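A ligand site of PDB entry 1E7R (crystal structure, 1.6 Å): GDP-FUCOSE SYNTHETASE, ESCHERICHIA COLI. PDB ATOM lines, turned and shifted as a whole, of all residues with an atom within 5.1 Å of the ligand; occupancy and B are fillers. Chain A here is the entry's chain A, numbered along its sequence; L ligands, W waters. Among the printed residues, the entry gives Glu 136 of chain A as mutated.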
ATOM      1  N   GLY A  10      11.354  14.667 -26.795  1.00  0.00           N
ATOM      2  CA  GLY A  10      11.491  15.938 -26.073  1.00  0.00           C
ATOM      3  C   GLY A  10      10.203  16.745 -26.118  1.00  0.00           C
ATOM      4  O   GLY A  10      10.194  17.965 -26.156  1.00  0.00           O
ATOM      5  N   ARG A  12       8.058  17.663 -23.917  1.00  0.00           N
ATOM      6  CA  ARG A  12       7.761  18.641 -22.867  1.00  0.00           C
ATOM      7  C   ARG A  12       8.689  19.869 -22.991  1.00  0.00           C
ATOM      8  O   ARG A  12       8.520  20.871 -22.308  1.00  0.00           O
ATOM      9  CB  ARG A  12       7.919  18.064 -21.455  1.00  0.00           C
ATOM     10  CG  ARG A  12       6.789  17.097 -21.139  1.00  0.00           C
ATOM     11  CD  ARG A  12       6.910  16.497 -19.766  1.00  0.00           C
ATOM     12  NE  ARG A  12       5.601  15.924 -19.405  1.00  0.00           N
ATOM     13  CZ  ARG A  12       5.393  15.391 -18.200  1.00  0.00           C
ATOM     14  NH1 ARG A  12       6.404  15.365 -17.356  1.00  0.00           N
ATOM     15  NH2 ARG A  12       4.222  14.866 -17.944  1.00  0.00           N
ATOM     16  N   GLY A  13       9.593  19.811 -23.974  1.00  0.00           N
ATOM     17  CA  GLY A  13      10.451  20.975 -24.198  1.00  0.00           C
ATOM     18  C   GLY A  13       9.706  22.150 -24.840  1.00  0.00           C
ATOM     19  O   GLY A  13       8.522  22.083 -25.219  1.00  0.00           O
ATOM     20  N   MET A  14      10.468  23.229 -24.986  1.00  0.00           N
ATOM     21  CA  MET A  14       9.876  24.435 -25.581  1.00  0.00           C
ATOM     22  C   MET A  14       9.391  24.142 -26.996  1.00  0.00           C
ATOM     23  O   MET A  14       8.260  24.406 -27.405  1.00  0.00           O
ATOM     24  CB  MET A  14      10.858  25.584 -25.449  1.00  0.00           C
ATOM     25  CG  MET A  14      10.316  26.875 -26.039  1.00  0.00           C
ATOM     26  SD  MET A  14      11.456  28.242 -25.699  1.00  0.00           S
ATOM     27  CE  MET A  14      10.752  29.506 -26.691  1.00  0.00           C
ATOM     28  N   VAL A  15      10.304  23.704 -27.869  1.00  0.00           N
ATOM     29  CA  VAL A  15      10.037  23.382 -29.246  1.00  0.00           C
ATOM     30  C   VAL A  15       9.148  22.149 -29.327  1.00  0.00           C
ATOM     31  O   VAL A  15       8.147  22.150 -30.050  1.00  0.00           O
ATOM     32  CB  VAL A  15      11.336  23.154 -30.038  1.00  0.00           C
ATOM     33  CG1 VAL A  15      11.056  22.686 -31.447  1.00  0.00           C
ATOM     34  CG2 VAL A  15      12.214  24.437 -30.059  1.00  0.00           C
ATOM     35  N   GLY A  16       9.468  21.051 -28.636  1.00  0.00           N
ATOM     36  CA  GLY A  16       8.664  19.825 -28.673  1.00  0.00           C
ATOM     37  C   GLY A  16       7.199  20.080 -28.338  1.00  0.00           C
ATOM     38  O   GLY A  16       6.324  19.500 -28.998  1.00  0.00           O
ATOM     39  N   ARG A  36      11.061  12.070 -19.972  1.00  0.00           N
ATOM     40  CA  ARG A  36      12.429  11.688 -19.657  1.00  0.00           C
ATOM     41  C   ARG A  36      12.485  10.523 -18.673  1.00  0.00           C
ATOM     42  O   ARG A  36      13.216   9.537 -18.829  1.00  0.00           O
ATOM     43  CB  ARG A  36      13.275  12.877 -19.184  1.00  0.00           C
ATOM     44  CG  ARG A  36      14.711  12.384 -18.966  1.00  0.00           C
ATOM     45  CD  ARG A  36      15.726  13.539 -18.936  1.00  0.00           C
ATOM     46  NE  ARG A  36      17.069  12.975 -18.714  1.00  0.00           N
ATOM     47  CZ  ARG A  36      18.149  13.758 -18.898  1.00  0.00           C
ATOM     48  NH1 ARG A  36      17.903  14.993 -19.306  1.00  0.00           N
ATOM     49  NH2 ARG A  36      19.382  13.289 -18.662  1.00  0.00           N
ATOM     50  N   LEU A  39      11.582   7.381 -20.577  1.00  0.00           N
ATOM     51  CA  LEU A  39      12.549   6.921 -21.578  1.00  0.00           C
ATOM     52  C   LEU A  39      13.742   7.864 -21.591  1.00  0.00           C
ATOM     53  O   LEU A  39      13.580   8.997 -22.037  1.00  0.00           O
ATOM     54  CB  LEU A  39      11.890   6.848 -22.955  1.00  0.00           C
ATOM     55  CG  LEU A  39      12.781   6.603 -24.178  1.00  0.00           C
ATOM     56  CD1 LEU A  39      13.544   5.295 -24.013  1.00  0.00           C
ATOM     57  CD2 LEU A  39      12.006   6.632 -25.483  1.00  0.00           C
ATOM     58  N   ASN A  40      14.899   7.377 -21.150  1.00  0.00           N
ATOM     59  CA  ASN A  40      16.112   8.196 -21.181  1.00  0.00           C
ATOM     60  C   ASN A  40      16.756   7.979 -22.557  1.00  0.00           C
ATOM     61  O   ASN A  40      17.246   6.865 -22.900  1.00  0.00           O
ATOM     62  CB  ASN A  40      17.055   7.689 -20.086  1.00  0.00           C
ATOM     63  CG  ASN A  40      18.379   8.415 -19.956  1.00  0.00           C
ATOM     64  OD1 ASN A  40      19.254   8.050 -19.128  1.00  0.00           O
ATOM     65  ND2 ASN A  40      18.581   9.316 -20.860  1.00  0.00           N
ATOM     66  N   LEU A  41      16.772   9.046 -23.358  1.00  0.00           N
ATOM     67  CA  LEU A  41      17.197   8.928 -24.749  1.00  0.00           C
ATOM     68  C   LEU A  41      18.718   8.764 -24.881  1.00  0.00           C
ATOM     69  O   LEU A  41      19.168   8.522 -25.987  1.00  0.00           O
ATOM     70  CB  LEU A  41      16.736  10.208 -25.508  1.00  0.00           C
ATOM     71  CG  LEU A  41      15.187  10.306 -25.582  1.00  0.00           C
ATOM     72  CD1 LEU A  41      14.842  11.718 -26.060  1.00  0.00           C
ATOM     73  CD2 LEU A  41      14.564   9.266 -26.503  1.00  0.00           C
ATOM     74  N   LEU A  42      19.448   8.927 -23.776  1.00  0.00           N
ATOM     75  CA  LEU A  42      20.885   8.590 -23.726  1.00  0.00           C
ATOM     76  C   LEU A  42      21.148   7.104 -23.668  1.00  0.00           C
ATOM     77  O   LEU A  42      22.256   6.641 -23.968  1.00  0.00           O
ATOM     78  CB  LEU A  42      21.492   9.243 -22.478  1.00  0.00           C
ATOM     79  CG  LEU A  42      21.514  10.792 -22.546  1.00  0.00           C
ATOM     80  CD1 LEU A  42      21.887  11.332 -21.142  1.00  0.00           C
ATOM     81  CD2 LEU A  42      22.498  11.304 -23.608  1.00  0.00           C
ATOM     82  N   ALA A  62      13.213  16.543 -31.098  1.00  0.00           N
ATOM     83  CA  ALA A  62      13.222  17.815 -30.380  1.00  0.00           C
ATOM     84  C   ALA A  62      13.799  17.687 -28.989  1.00  0.00           C
ATOM     85  O   ALA A  62      13.653  18.589 -28.176  1.00  0.00           O
ATOM     86  CB  ALA A  62      11.845  18.494 -30.404  1.00  0.00           C
ATOM     87  N   ALA A  63      14.408  16.573 -28.625  1.00  0.00           N
ATOM     88  CA  ALA A  63      15.116  16.394 -27.354  1.00  0.00           C
ATOM     89  C   ALA A  63      16.598  16.744 -27.462  1.00  0.00           C
ATOM     90  O   ALA A  63      17.224  16.442 -28.488  1.00  0.00           O
ATOM     91  CB  ALA A  63      15.057  14.936 -26.919  1.00  0.00           C
ATOM     92  N   ALA A  64      17.098  17.491 -26.500  1.00  0.00           N
ATOM     93  CA  ALA A  64      18.530  17.894 -26.580  1.00  0.00           C
ATOM     94  C   ALA A  64      18.900  18.458 -25.219  1.00  0.00           C
ATOM     95  O   ALA A  64      18.041  18.761 -24.376  1.00  0.00           O
ATOM     96  CB  ALA A  64      18.712  19.019 -27.603  1.00  0.00           C
ATOM     97  N   LYS A  65      20.178  18.452 -24.923  1.00  0.00           N
ATOM     98  CA  LYS A  65      20.714  19.218 -23.781  1.00  0.00           C
ATOM     99  C   LYS A  65      20.910  20.647 -24.265  1.00  0.00           C
ATOM    100  O   LYS A  65      21.632  20.918 -25.281  1.00  0.00           O
ATOM    101  CB  LYS A  65      22.046  18.517 -23.446  1.00  0.00           C
ATOM    102  CG  LYS A  65      22.856  19.307 -22.450  1.00  0.00           C
ATOM    103  CD  LYS A  65      22.105  19.437 -21.173  1.00  0.00           C
ATOM    104  CE  LYS A  65      23.034  19.915 -20.066  1.00  0.00           C
ATOM    105  NZ  LYS A  65      22.341  20.015 -18.759  1.00  0.00           N
ATOM    106  N   VAL A  66      20.209  21.547 -23.599  1.00  0.00           N
ATOM    107  CA  VAL A  66      20.129  22.943 -24.082  1.00  0.00           C
ATOM    108  C   VAL A  66      20.457  23.846 -22.893  1.00  0.00           C
ATOM    109  O   VAL A  66      20.117  23.524 -21.727  1.00  0.00           O
ATOM    110  CB  VAL A  66      18.659  23.203 -24.543  1.00  0.00           C
ATOM    111  CG1 VAL A  66      18.384  24.622 -24.892  1.00  0.00           C
ATOM    112  CG2 VAL A  66      18.358  22.300 -25.715  1.00  0.00           C
ATOM    113  N   ILE A  86      22.047  11.347 -27.889  1.00  0.00           N
ATOM    114  CA  ILE A  86      20.580  11.377 -28.178  1.00  0.00           C
ATOM    115  C   ILE A  86      20.336  11.233 -29.674  1.00  0.00           C
ATOM    116  O   ILE A  86      19.470  10.434 -30.104  1.00  0.00           O
ATOM    117  CB  ILE A  86      19.954  12.649 -27.619  1.00  0.00           C
ATOM    118  CG1 ILE A  86      20.013  12.668 -26.103  1.00  0.00           C
ATOM    119  CG2 ILE A  86      18.551  12.924 -28.184  1.00  0.00           C
ATOM    120  CD1 ILE A  86      19.705  14.006 -25.451  1.00  0.00           C
ATOM    121  N   LEU A 105      15.705  18.668 -35.330  1.00  0.00           N
ATOM    122  CA  LEU A 105      15.759  20.093 -34.961  1.00  0.00           C
ATOM    123  C   LEU A 105      17.156  20.445 -34.466  1.00  0.00           C
ATOM    124  O   LEU A 105      17.526  19.925 -33.397  1.00  0.00           O
ATOM    125  CB  LEU A 105      14.819  20.340 -33.784  1.00  0.00           C
ATOM    126  CG  LEU A 105      13.336  20.464 -34.021  1.00  0.00           C
ATOM    127  CD1 LEU A 105      12.923  21.768 -34.603  1.00  0.00           C
ATOM    128  CD2 LEU A 105      12.704  19.352 -34.826  1.00  0.00           C
ATOM    129  N   GLY A 106      17.851  21.276 -35.253  1.00  0.00           N
ATOM    130  CA  GLY A 106      19.173  21.713 -34.906  1.00  0.00           C
ATOM    131  C   GLY A 106      19.086  23.123 -34.330  1.00  0.00           C
ATOM    132  O   GLY A 106      18.147  23.483 -33.641  1.00  0.00           O
ATOM    133  N   SER A 107      20.016  23.956 -34.723  1.00  0.00           N
ATOM    134  CA  SER A 107      20.069  25.350 -34.268  1.00  0.00           C
ATOM    135  C   SER A 107      20.931  26.196 -35.170  1.00  0.00           C
ATOM    136  O   SER A 107      21.736  25.681 -35.923  1.00  0.00           O
ATOM    137  CB  SER A 107      20.750  25.307 -32.876  1.00  0.00           C
ATOM    138  OG  SER A 107      21.019  26.636 -32.583  1.00  0.00           O
ATOM    139  N   SER A 108      20.764  27.504 -35.220  1.00  0.00           N
ATOM    140  CA  SER A 108      21.599  28.370 -36.053  1.00  0.00           C
ATOM    141  C   SER A 108      22.997  28.498 -35.451  1.00  0.00           C
ATOM    142  O   SER A 108      23.827  29.125 -36.130  1.00  0.00           O
ATOM    143  CB  SER A 108      20.943  29.724 -36.289  1.00  0.00           C
ATOM    144  OG  SER A 108      20.639  30.292 -35.031  1.00  0.00           O
ATOM    145  N   GLU A 136      28.379  22.076 -28.610  1.00  0.00           N
ATOM    146  CA  GLU A 136      27.031  21.753 -28.995  1.00  0.00           C
ATOM    147  C   GLU A 136      26.878  21.838 -30.513  1.00  0.00           C
ATOM    148  O   GLU A 136      26.140  21.048 -31.110  1.00  0.00           O
ATOM    149  CB  GLU A 136      26.165  22.839 -28.314  1.00  0.00           C
ATOM    150  CG  GLU A 136      24.929  23.243 -28.980  1.00  0.00           C
ATOM    151  CD  GLU A 136      24.250  24.375 -28.247  1.00  0.00           C
ATOM    152  OE1 GLU A 136      24.491  25.601 -28.471  1.00  0.00           O
ATOM    153  OE2 GLU A 136      23.366  23.914 -27.474  1.00  0.00           O
ATOM    154  N   LYS A 140      25.446  19.075 -33.138  1.00  0.00           N
ATOM    155  CA  LYS A 140      24.295  19.267 -34.035  1.00  0.00           C
ATOM    156  C   LYS A 140      24.668  19.118 -35.485  1.00  0.00           C
ATOM    157  O   LYS A 140      23.915  18.490 -36.268  1.00  0.00           O
ATOM    158  CB  LYS A 140      23.663  20.633 -33.774  1.00  0.00           C
ATOM    159  CG  LYS A 140      23.001  20.697 -32.386  1.00  0.00           C
ATOM    160  CD  LYS A 140      22.474  22.054 -32.053  1.00  0.00           C
ATOM    161  CE  LYS A 140      22.127  22.265 -30.571  1.00  0.00           C
ATOM    162  NZ  LYS A 140      21.035  21.264 -30.262  1.00  0.00           N
ATOM    163  N   PRO A 163      16.493  26.329 -36.664  1.00  0.00           N
ATOM    164  CA  PRO A 163      15.802  27.533 -36.226  1.00  0.00           C
ATOM    165  C   PRO A 163      16.749  28.663 -35.884  1.00  0.00           C
ATOM    166  O   PRO A 163      17.821  28.419 -35.334  1.00  0.00           O
ATOM    167  CB  PRO A 163      15.134  27.126 -34.924  1.00  0.00           C
ATOM    168  CG  PRO A 163      15.954  25.949 -34.461  1.00  0.00           C
ATOM    169  CD  PRO A 163      16.475  25.263 -35.676  1.00  0.00           C
ATOM    170  N   THR A 164      16.279  29.886 -36.022  1.00  0.00           N
ATOM    171  CA  THR A 164      16.896  31.082 -35.496  1.00  0.00           C
ATOM    172  C   THR A 164      16.554  31.181 -34.005  1.00  0.00           C
ATOM    173  O   THR A 164      16.099  30.214 -33.374  1.00  0.00           O
ATOM    174  CB  THR A 164      16.448  32.336 -36.284  1.00  0.00           C
ATOM    175  OG1 THR A 164      17.281  33.421 -36.023  1.00  0.00           O
ATOM    176  CG2 THR A 164      14.947  32.604 -36.102  1.00  0.00           C
ATOM    177  N   ASN A 165      16.832  32.337 -33.378  1.00  0.00           N
ATOM    178  CA  ASN A 165      16.506  32.549 -31.995  1.00  0.00           C
ATOM    179  C   ASN A 165      14.971  32.391 -31.849  1.00  0.00           C
ATOM    180  O   ASN A 165      14.263  33.077 -32.596  1.00  0.00           O
ATOM    181  CB  ASN A 165      16.874  33.980 -31.565  1.00  0.00           C
ATOM    182  CG  ASN A 165      18.368  34.222 -31.653  1.00  0.00           C
ATOM    183  OD1 ASN A 165      19.179  33.497 -31.065  1.00  0.00           O
ATOM    184  ND2 ASN A 165      18.743  35.143 -32.549  1.00  0.00           N
ATOM    185  N   LEU A 166      14.564  31.640 -30.859  1.00  0.00           N
ATOM    186  CA  LEU A 166      13.108  31.437 -30.656  1.00  0.00           C
ATOM    187  C   LEU A 166      12.678  32.031 -29.347  1.00  0.00           C
ATOM    188  O   LEU A 166      13.461  32.189 -28.421  1.00  0.00           O
ATOM    189  CB  LEU A 166      12.799  29.906 -30.614  1.00  0.00           C
ATOM    190  CG  LEU A 166      13.221  29.095 -31.811  1.00  0.00           C
ATOM    191  CD1 LEU A 166      12.824  27.617 -31.618  1.00  0.00           C
ATOM    192  CD2 LEU A 166      12.646  29.698 -33.132  1.00  0.00           C
ATOM    193  N   TYR A 167      11.374  32.310 -29.211  1.00  0.00           N
ATOM    194  CA  TYR A 167      10.796  32.807 -27.949  1.00  0.00           C
ATOM    195  C   TYR A 167       9.337  32.352 -27.960  1.00  0.00           C
ATOM    196  O   TYR A 167       8.820  31.924 -29.013  1.00  0.00           O
ATOM    197  CB  TYR A 167      10.924  34.335 -27.886  1.00  0.00           C
ATOM    198  CG  TYR A 167      10.113  35.039 -28.950  1.00  0.00           C
ATOM    199  CD1 TYR A 167      10.506  35.211 -30.261  1.00  0.00           C
ATOM    200  CD2 TYR A 167       8.847  35.522 -28.571  1.00  0.00           C
ATOM    201  CE1 TYR A 167       9.737  35.892 -31.201  1.00  0.00           C
ATOM    202  CE2 TYR A 167       8.101  36.200 -29.519  1.00  0.00           C
ATOM    203  CZ  TYR A 167       8.465  36.270 -30.845  1.00  0.00           C
ATOM    204  OH  TYR A 167       7.643  36.967 -31.703  1.00  0.00           O
ATOM    205  N   HIS A 179      19.418  34.360 -23.064  1.00  0.00           N
ATOM    206  CA  HIS A 179      18.545  34.625 -24.220  1.00  0.00           C
ATOM    207  C   HIS A 179      17.732  35.905 -23.993  1.00  0.00           C
ATOM    208  O   HIS A 179      17.080  36.056 -22.958  1.00  0.00           O
ATOM    209  CB  HIS A 179      17.581  33.520 -24.520  1.00  0.00           C
ATOM    210  CG  HIS A 179      18.068  32.200 -24.974  1.00  0.00           C
ATOM    211  ND1 HIS A 179      17.281  31.226 -25.551  1.00  0.00           N
ATOM    212  CD2 HIS A 179      19.298  31.720 -25.019  1.00  0.00           C
ATOM    213  CE1 HIS A 179      18.044  30.225 -25.931  1.00  0.00           C
ATOM    214  NE2 HIS A 179      19.302  30.494 -25.606  1.00  0.00           N
HETATM  215  P1  LIG L   1      13.808  22.489 -24.071  1.00  0.00           P
HETATM  216  O1  LIG L   1      14.471  23.327 -23.118  1.00  0.00           O
HETATM  217  O2  LIG L   1      12.872  22.892 -25.163  1.00  0.00           O
HETATM  218  O3  LIG L   1      14.076  20.889 -23.801  1.00  0.00           O
HETATM  219  C1  LIG L   1      13.931  19.906 -24.841  1.00  0.00           C
HETATM  220  C2  LIG L   1      13.815  18.688 -23.965  1.00  0.00           C
HETATM  221  O4  LIG L   1      14.205  17.419 -24.520  1.00  0.00           O
HETATM  222  C3  LIG L   1      13.841  18.749 -22.484  1.00  0.00           C
HETATM  223  O5  LIG L   1      12.491  18.654 -21.947  1.00  0.00           O
HETATM  224  C4  LIG L   1      14.614  17.562 -22.120  1.00  0.00           C
HETATM  225  O6  LIG L   1      14.402  16.850 -20.895  1.00  0.00           O
HETATM  226  C5  LIG L   1      14.427  16.678 -23.304  1.00  0.00           C
HETATM  227  N1  LIG L   1      15.585  15.772 -23.113  1.00  0.00           N
HETATM  228  C6  LIG L   1      16.938  16.112 -22.979  1.00  0.00           C
HETATM  229  N2  LIG L   1      17.665  15.055 -22.718  1.00  0.00           N
HETATM  230  C7  LIG L   1      16.838  13.971 -22.677  1.00  0.00           C
HETATM  231  C8  LIG L   1      17.044  12.653 -22.413  1.00  0.00           C
HETATM  232  N3  LIG L   1      18.258  12.189 -22.145  1.00  0.00           N
HETATM  233  N4  LIG L   1      15.995  11.836 -22.426  1.00  0.00           N
HETATM  234  C9  LIG L   1      14.785  12.327 -22.688  1.00  0.00           C
HETATM  235  N5  LIG L   1      14.494  13.577 -22.937  1.00  0.00           N
HETATM  236  C10 LIG L   1      15.576  14.389 -22.929  1.00  0.00           C
HETATM  237  O7  LIG L   1      14.684  22.552 -25.401  1.00  0.00           O
HETATM  238  P2  LIG L   1      14.321  23.559 -26.621  1.00  0.00           P
HETATM  239  O8  LIG L   1      14.576  24.893 -26.031  1.00  0.00           O
HETATM  240  O9  LIG L   1      12.928  23.178 -27.044  1.00  0.00           O
HETATM  241  O10 LIG L   1      15.237  23.212 -27.864  1.00  0.00           O
HETATM  242  C11 LIG L   1      14.996  21.940 -28.561  1.00  0.00           C
HETATM  243  C12 LIG L   1      15.931  21.935 -29.782  1.00  0.00           C
HETATM  244  O11 LIG L   1      15.608  23.139 -30.453  1.00  0.00           O
HETATM  245  C13 LIG L   1      17.359  22.087 -29.296  1.00  0.00           C
HETATM  246  O12 LIG L   1      18.183  21.153 -29.970  1.00  0.00           O
HETATM  247  C14 LIG L   1      17.714  23.489 -29.550  1.00  0.00           C
HETATM  248  O13 LIG L   1      19.106  23.588 -29.833  1.00  0.00           O
HETATM  249  C15 LIG L   1      16.793  23.808 -30.790  1.00  0.00           C
HETATM  250  N6  LIG L   1      16.690  25.247 -30.704  1.00  0.00           N
HETATM  251  C16 LIG L   1      15.929  25.836 -29.686  1.00  0.00           C
HETATM  252  C17 LIG L   1      15.912  27.275 -29.638  1.00  0.00           C
HETATM  253  C18 LIG L   1      15.135  28.027 -28.619  1.00  0.00           C
HETATM  254  O14 LIG L   1      14.400  27.476 -27.772  1.00  0.00           O
HETATM  255  N7  LIG L   1      15.184  29.368 -28.615  1.00  0.00           N
HETATM  256  C19 LIG L   1      16.652  27.952 -30.580  1.00  0.00           C
HETATM  257  C20 LIG L   1      17.379  27.343 -31.537  1.00  0.00           C
HETATM  258  C21 LIG L   1      17.387  25.989 -31.599  1.00  0.00           C
HETATM  259  P3  LIG L   1      14.535  17.355 -19.433  1.00  0.00           P
HETATM  260  O15 LIG L   1      13.278  17.399 -18.673  1.00  0.00           O
HETATM  261  O16 LIG L   1      15.863  17.829 -18.937  1.00  0.00           O
HETATM  262  O17 LIG L   1      14.248  18.773 -19.921  1.00  0.00           O
HETATM  263  O   HOH W   1      18.476  18.196 -20.371  1.00  0.00           O
HETATM  264  O   HOH W   2      10.365  16.187 -22.833  1.00  0.00           O
HETATM  265  O   HOH W   3      20.687  25.874 -28.806  1.00  0.00           O
HETATM  266  O   HOH W   4      14.647  26.452 -23.987  1.00  0.00           O
HETATM  267  O   HOH W   5      11.845  20.614 -27.206  1.00  0.00           O
HETATM  268  O   HOH W   6      11.853  10.611 -23.414  1.00  0.00           O
HETATM  269  O   HOH W   7      16.871  18.629 -30.796  1.00  0.00           O
HETATM  270  O   HOH W   8      11.688  13.965 -23.405  1.00  0.00           O
HETATM  271  O   HOH W   9      11.970  23.613 -21.456  1.00  0.00           O
HETATM  272  O   HOH W  10      20.251  14.377 -21.670  1.00  0.00           O
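Water W5 lies within hydrogen-bond range of an oxygen (O9) of the ligand (2.8 Å), the backbone NH of Gly 16 (2.8 Å), the backbone carbonyl oxygen of Ala 62 (2.9 Å) and the backbone carbonyl oxygen of Gly 10 (3.3 Å).
Water W8 bridges a nitrogen (N5) of the ligand (2.9 Å) and the backbone NH (N) of Gly 10 (3.5 Å).
Water W10 lies within hydrogen-bond range of a nitrogen (N2) of the ligand (2.9 Å) and the guanidinium group (NH2) of Arg 36 (3.3 Å).
Water W7 lies within hydrogen-bond range of an oxygen (O12) of the ligand, the backbone carbonyl oxygen of Leu 105 and the backbone carbonyl oxygen of Ala 63.
Water W1 bridges an oxygen (O16) of the ligand and the guanidinium group (NH1) of Arg 36.
Water W2 bridges the backbone NH (N) of Arg 12 and an oxygen (O5) of the ligand.
Residues that only touch the ligand: Ala 63 (3.1 Å), Gly 106 (3.2 Å), Ala 64 (3.2 Å), Pro 163 (3.2 Å), Gly 13 (3.2 Å), Gly 10 (3.5 Å), Leu 42 (3.6 Å), Ile 86 (3.6 Å), Ala 62 (3.6 Å), Leu 39 (3.6 Å), Thr 164 (3.6 Å), Ser 107 (3.7 Å), Val 66 (3.7 Å) and Leu 105 (3.7 Å).
Hydrophobic or aromatic side chains within 4 Å of the ligand: Met 14, Val 15, Leu 41, Leu 42, Ala 63, Ala 64, Val 66, Ile 86, Pro 163 and Leu 166.
N of Met 14 is in hydrogen-bond range of O2 of the ligand (2.4 Å).
N of Val 15 sits at hydrogen-bond distance from O9 of the ligand (2.8 Å).
An oxygen (O12) of the ligand lies within hydrogen-bond range of the side-chain amino group of Lys 140 (2.9 Å).
A nitrogen (N4) of the ligand lies within hydrogen-bond range of the backbone NH (N) of Leu 41 (3.0 Å).
A nitrogen (N7) of the ligand sits close to the backbone carbonyl oxygen (O) of Leu 166.
The side-chain amide nitrogen (ND2) of Asn 40 sits close to a nitrogen (N3) of the ligand (3.2 Å).
NH1 of Arg 36 lies within salt-bridge range of O16 of the ligand, at 3.5 Å.
ND2 of Asn 40 lies close to N of Leu 42 (3.1 Å).
The backbone carbonyl oxygen (O) of Pro 163 is in hydrogen-bond range of the backbone NH (N) of Ser 108 (3.1 Å).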
